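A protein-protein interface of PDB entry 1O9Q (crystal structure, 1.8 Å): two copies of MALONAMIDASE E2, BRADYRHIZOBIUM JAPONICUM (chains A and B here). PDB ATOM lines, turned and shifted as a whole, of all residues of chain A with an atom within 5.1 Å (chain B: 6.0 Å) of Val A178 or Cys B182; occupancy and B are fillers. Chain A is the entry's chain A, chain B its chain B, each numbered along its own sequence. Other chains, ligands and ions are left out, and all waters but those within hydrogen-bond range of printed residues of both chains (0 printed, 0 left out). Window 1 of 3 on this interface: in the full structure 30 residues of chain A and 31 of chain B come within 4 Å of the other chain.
Val A178 touches one residue of chain B. Of chain A, only Val A178 (3.6 Å) comes within 4 Å of Cys B182. Of the printed residues of chain A, Trp B185 touches Pro A176. Of the printed residues of chain B, Pro A176 touches Trp B185 (3.7 Å). Val A180 touches none of the printed residues of chain B. Phe B110 touches none of the printed residues of chain A. The nearest printed residue of chain A that does not touch Cys B182 is Pro A176 (6.8 Å). The nearest printed residue of chain B that does not touch Pro A89 is Leu B285 (5.2 Å).
The backbone NH of Ser B184 lies within hydrogen-bond range of the side-chain sulfur of Cys B182 (3.8 Å). The side-chain sulfur of Cys B182 is in hydrogen-bond range of the backbone NH of Trp B185 (3.5 Å). SG of Cys B182 lies close to OD2 of Asp B188.
Among the printed residues, merely in contact across the chains: Pro A89 with Ala B284 (3.9 Å), Pro A176 with Trp B185 (3.7 Å) and Val A178 with Cys B182 (3.6 Å).
1 position is printed for both chains.
Of the 10 printed residues of chain B, 3 touch a printed residue of chain A. Printed residues of chain B that touch a printed residue of chain A: Cys B182, Trp B185 and Ala B284. Hydrophobic or aromatic side chains of chain B within 4 Å of the printed part of chain A: Trp B185. Among the printed residues, no Asp or Glu carboxylate lies within 4 Å of a Lys or Arg side-chain nitrogen of the other chain.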
ATOM      1  N   ALA A  88       3.203 -12.245 -19.307  1.00  0.00           N
ATOM      2  CA  ALA A  88       4.081 -11.291 -19.975  1.00  0.00           C
ATOM      3  C   ALA A  88       3.274 -10.562 -21.045  1.00  0.00           C
ATOM      4  O   ALA A  88       2.297 -11.091 -21.569  1.00  0.00           O
ATOM      5  CB  ALA A  88       5.261 -12.019 -20.611  1.00  0.00           C
ATOM      6  N   PRO A  89       3.659  -9.324 -21.362  1.00  0.00           N
ATOM      7  CA  PRO A  89       2.917  -8.594 -22.387  1.00  0.00           C
ATOM      8  C   PRO A  89       2.726  -9.360 -23.716  1.00  0.00           C
ATOM      9  O   PRO A  89       1.665  -9.264 -24.330  1.00  0.00           O
ATOM     10  CB  PRO A  89       3.734  -7.321 -22.536  1.00  0.00           C
ATOM     11  CG  PRO A  89       4.100  -7.040 -21.091  1.00  0.00           C
ATOM     12  CD  PRO A  89       4.539  -8.414 -20.603  1.00  0.00           C
ATOM     13  N   PRO A 176       7.636  -6.447 -26.988  1.00  0.00           N
ATOM     14  CA  PRO A 176       8.251  -6.206 -25.680  1.00  0.00           C
ATOM     15  C   PRO A 176       8.865  -7.449 -25.030  1.00  0.00           C
ATOM     16  O   PRO A 176       8.349  -8.559 -25.174  1.00  0.00           O
ATOM     17  CB  PRO A 176       7.095  -5.637 -24.861  1.00  0.00           C
ATOM     18  CG  PRO A 176       5.905  -6.361 -25.431  1.00  0.00           C
ATOM     19  CD  PRO A 176       6.168  -6.312 -26.920  1.00  0.00           C
ATOM     20  N   THR A 177       9.974  -7.253 -24.322  1.00  0.00           N
ATOM     21  CA  THR A 177      10.628  -8.359 -23.618  1.00  0.00           C
ATOM     22  C   THR A 177      10.280  -8.272 -22.127  1.00  0.00           C
ATOM     23  O   THR A 177      10.910  -8.917 -21.293  1.00  0.00           O
ATOM     24  CB  THR A 177      12.157  -8.337 -23.800  1.00  0.00           C
ATOM     25  OG1 THR A 177      12.659  -7.027 -23.518  1.00  0.00           O
ATOM     26  CG2 THR A 177      12.523  -8.735 -25.230  1.00  0.00           C
ATOM     27  N   VAL A 178       9.279  -7.452 -21.806  1.00  0.00           N
ATOM     28  CA  VAL A 178       8.806  -7.326 -20.420  1.00  0.00           C
ATOM     29  C   VAL A 178       8.285  -8.728 -20.067  1.00  0.00           C
ATOM     30  O   VAL A 178       7.588  -9.348 -20.867  1.00  0.00           O
ATOM     31  CB  VAL A 178       7.633  -6.316 -20.309  1.00  0.00           C
ATOM     32  CG1 VAL A 178       6.990  -6.397 -18.917  1.00  0.00           C
ATOM     33  CG2 VAL A 178       8.133  -4.906 -20.571  1.00  0.00           C
ATOM     34  N   GLY A 179       8.637  -9.226 -18.887  1.00  0.00           N
ATOM     35  CA  GLY A 179       8.182 -10.542 -18.490  1.00  0.00           C
ATOM     36  C   GLY A 179       8.920 -11.670 -19.193  1.00  0.00           C
ATOM     37  O   GLY A 179       8.454 -12.810 -19.198  1.00  0.00           O
ATOM     38  N   VAL A 180      10.065 -11.354 -19.791  1.00  0.00           N
ATOM     39  CA  VAL A 180      10.890 -12.354 -20.491  1.00  0.00           C
ATOM     40  C   VAL A 180      12.258 -12.387 -19.791  1.00  0.00           C
ATOM     41  O   VAL A 180      12.987 -11.398 -19.809  1.00  0.00           O
ATOM     42  CB  VAL A 180      11.089 -11.969 -21.972  1.00  0.00           C
ATOM     43  CG1 VAL A 180      11.947 -13.013 -22.677  1.00  0.00           C
ATOM     44  CG2 VAL A 180       9.730 -11.838 -22.662  1.00  0.00           C
ATOM     45  N   PHE B 110       2.193   1.533  -9.951  1.00  0.00           N
ATOM     46  CA  PHE B 110       2.848   1.318 -11.246  1.00  0.00           C
ATOM     47  C   PHE B 110       3.599   2.569 -11.750  1.00  0.00           C
ATOM     48  O   PHE B 110       3.713   2.801 -12.955  1.00  0.00           O
ATOM     49  CB  PHE B 110       1.798   0.859 -12.261  1.00  0.00           C
ATOM     50  CG  PHE B 110       1.060  -0.377 -11.836  1.00  0.00           C
ATOM     51  CD1 PHE B 110      -0.251  -0.299 -11.381  1.00  0.00           C
ATOM     52  CD2 PHE B 110       1.695  -1.618 -11.844  1.00  0.00           C
ATOM     53  CE1 PHE B 110      -0.921  -1.439 -10.936  1.00  0.00           C
ATOM     54  CE2 PHE B 110       1.035  -2.761 -11.399  1.00  0.00           C
ATOM     55  CZ  PHE B 110      -0.276  -2.671 -10.945  1.00  0.00           C
ATOM     56  N   VAL B 180      12.670  -4.245 -13.105  1.00  0.00           N
ATOM     57  CA  VAL B 180      12.058  -2.941 -12.813  1.00  0.00           C
ATOM     58  C   VAL B 180      10.704  -2.948 -13.524  1.00  0.00           C
ATOM     59  O   VAL B 180      10.648  -3.031 -14.747  1.00  0.00           O
ATOM     60  CB  VAL B 180      12.918  -1.772 -13.352  1.00  0.00           C
ATOM     61  CG1 VAL B 180      12.264  -0.437 -13.010  1.00  0.00           C
ATOM     62  CG2 VAL B 180      14.315  -1.837 -12.752  1.00  0.00           C
ATOM     63  N   LYS B 181       9.622  -2.885 -12.751  1.00  0.00           N
ATOM     64  CA  LYS B 181       8.268  -2.910 -13.318  1.00  0.00           C
ATOM     65  C   LYS B 181       8.166  -1.890 -14.438  1.00  0.00           C
ATOM     66  O   LYS B 181       8.297  -0.688 -14.213  1.00  0.00           O
ATOM     67  CB  LYS B 181       7.253  -2.603 -12.216  1.00  0.00           C
ATOM     68  CG  LYS B 181       5.797  -2.713 -12.651  1.00  0.00           C
ATOM     69  CD  LYS B 181       5.486  -4.070 -13.251  1.00  0.00           C
ATOM     70  CE  LYS B 181       3.976  -4.259 -13.427  1.00  0.00           C
ATOM     71  NZ  LYS B 181       3.681  -5.398 -14.331  1.00  0.00           N
ATOM     72  N   CYS B 182       7.920  -2.380 -15.645  1.00  0.00           N
ATOM     73  CA  CYS B 182       7.850  -1.514 -16.809  1.00  0.00           C
ATOM     74  C   CYS B 182       6.553  -0.744 -17.036  1.00  0.00           C
ATOM     75  O   CYS B 182       5.451  -1.268 -16.846  1.00  0.00           O
ATOM     76  CB  CYS B 182       8.163  -2.356 -18.047  1.00  0.00           C
ATOM     77  SG  CYS B 182       8.124  -1.423 -19.608  1.00  0.00           S
ATOM     78  N   TYR B 183       6.710   0.513 -17.440  1.00  0.00           N
ATOM     79  CA  TYR B 183       5.571   1.363 -17.776  1.00  0.00           C
ATOM     80  C   TYR B 183       5.734   1.659 -19.279  1.00  0.00           C
ATOM     81  O   TYR B 183       4.814   1.451 -20.066  1.00  0.00           O
ATOM     82  CB  TYR B 183       5.596   2.653 -16.959  1.00  0.00           C
ATOM     83  CG  TYR B 183       4.325   3.455 -17.127  1.00  0.00           C
ATOM     84  CD1 TYR B 183       4.147   4.299 -18.221  1.00  0.00           C
ATOM     85  CD2 TYR B 183       3.282   3.336 -16.213  1.00  0.00           C
ATOM     86  CE1 TYR B 183       2.963   5.002 -18.400  1.00  0.00           C
ATOM     87  CE2 TYR B 183       2.095   4.035 -16.382  1.00  0.00           C
ATOM     88  CZ  TYR B 183       1.942   4.867 -17.478  1.00  0.00           C
ATOM     89  OH  TYR B 183       0.771   5.574 -17.638  1.00  0.00           O
ATOM     90  N   SER B 184       6.919   2.140 -19.650  1.00  0.00           N
ATOM     91  CA  SER B 184       7.267   2.423 -21.054  1.00  0.00           C
ATOM     92  C   SER B 184       8.741   2.017 -21.222  1.00  0.00           C
ATOM     93  O   SER B 184       9.634   2.659 -20.670  1.00  0.00           O
ATOM     94  CB  SER B 184       7.099   3.913 -21.362  1.00  0.00           C
ATOM     95  OG  SER B 184       7.561   4.202 -22.674  1.00  0.00           O
ATOM     96  N   TRP B 185       8.986   0.947 -21.972  1.00  0.00           N
ATOM     97  CA  TRP B 185      10.361   0.473 -22.162  1.00  0.00           C
ATOM     98  C   TRP B 185      11.219   1.426 -22.979  1.00  0.00           C
ATOM     99  O   TRP B 185      12.442   1.353 -22.954  1.00  0.00           O
ATOM    100  CB  TRP B 185      10.335  -0.932 -22.785  1.00  0.00           C
ATOM    101  CG  TRP B 185       9.674  -1.047 -24.130  1.00  0.00           C
ATOM    102  CD1 TRP B 185      10.248  -0.826 -25.352  1.00  0.00           C
ATOM    103  CD2 TRP B 185       8.320  -1.447 -24.391  1.00  0.00           C
ATOM    104  NE1 TRP B 185       9.340  -1.072 -26.356  1.00  0.00           N
ATOM    105  CE2 TRP B 185       8.148  -1.455 -25.795  1.00  0.00           C
ATOM    106  CE3 TRP B 185       7.237  -1.804 -23.575  1.00  0.00           C
ATOM    107  CZ2 TRP B 185       6.931  -1.803 -26.401  1.00  0.00           C
ATOM    108  CZ3 TRP B 185       6.028  -2.151 -24.178  1.00  0.00           C
ATOM    109  CH2 TRP B 185       5.888  -2.150 -25.579  1.00  0.00           C
ATOM    110  N   ASP B 188      11.455   4.320 -19.474  1.00  0.00           N
ATOM    111  CA  ASP B 188      11.928   3.887 -18.146  1.00  0.00           C
ATOM    112  C   ASP B 188      13.451   3.936 -17.985  1.00  0.00           C
ATOM    113  O   ASP B 188      14.193   3.308 -18.741  1.00  0.00           O
ATOM    114  CB  ASP B 188      11.430   2.466 -17.865  1.00  0.00           C
ATOM    115  CG  ASP B 188       9.920   2.389 -17.705  1.00  0.00           C
ATOM    116  OD1 ASP B 188       9.238   3.432 -17.836  1.00  0.00           O
ATOM    117  OD2 ASP B 188       9.416   1.274 -17.443  1.00  0.00           O
ATOM    118  N   ALA B 284       2.621  -2.920 -21.796  1.00  0.00           N
ATOM    119  CA  ALA B 284       3.368  -3.278 -20.569  1.00  0.00           C
ATOM    120  C   ALA B 284       2.485  -3.633 -19.370  1.00  0.00           C
ATOM    121  O   ALA B 284       2.892  -4.398 -18.492  1.00  0.00           O
ATOM    122  CB  ALA B 284       4.314  -2.142 -20.188  1.00  0.00           C
ATOM    123  N   LEU B 285       1.288  -3.065 -19.331  1.00  0.00           N
ATOM    124  CA  LEU B 285       0.352  -3.328 -18.232  1.00  0.00           C
ATOM    125  C   LEU B 285      -0.886  -4.062 -18.755  1.00  0.00           C
ATOM    126  O   LEU B 285      -1.964  -3.961 -18.177  1.00  0.00           O
ATOM    127  CB  LEU B 285      -0.047  -1.989 -17.596  1.00  0.00           C
ATOM    128  CG  LEU B 285       1.073  -1.168 -16.951  1.00  0.00           C
ATOM    129  CD1 LEU B 285       0.563   0.228 -16.580  1.00  0.00           C
ATOM    130  CD2 LEU B 285       1.590  -1.902 -15.725  1.00  0.00           C
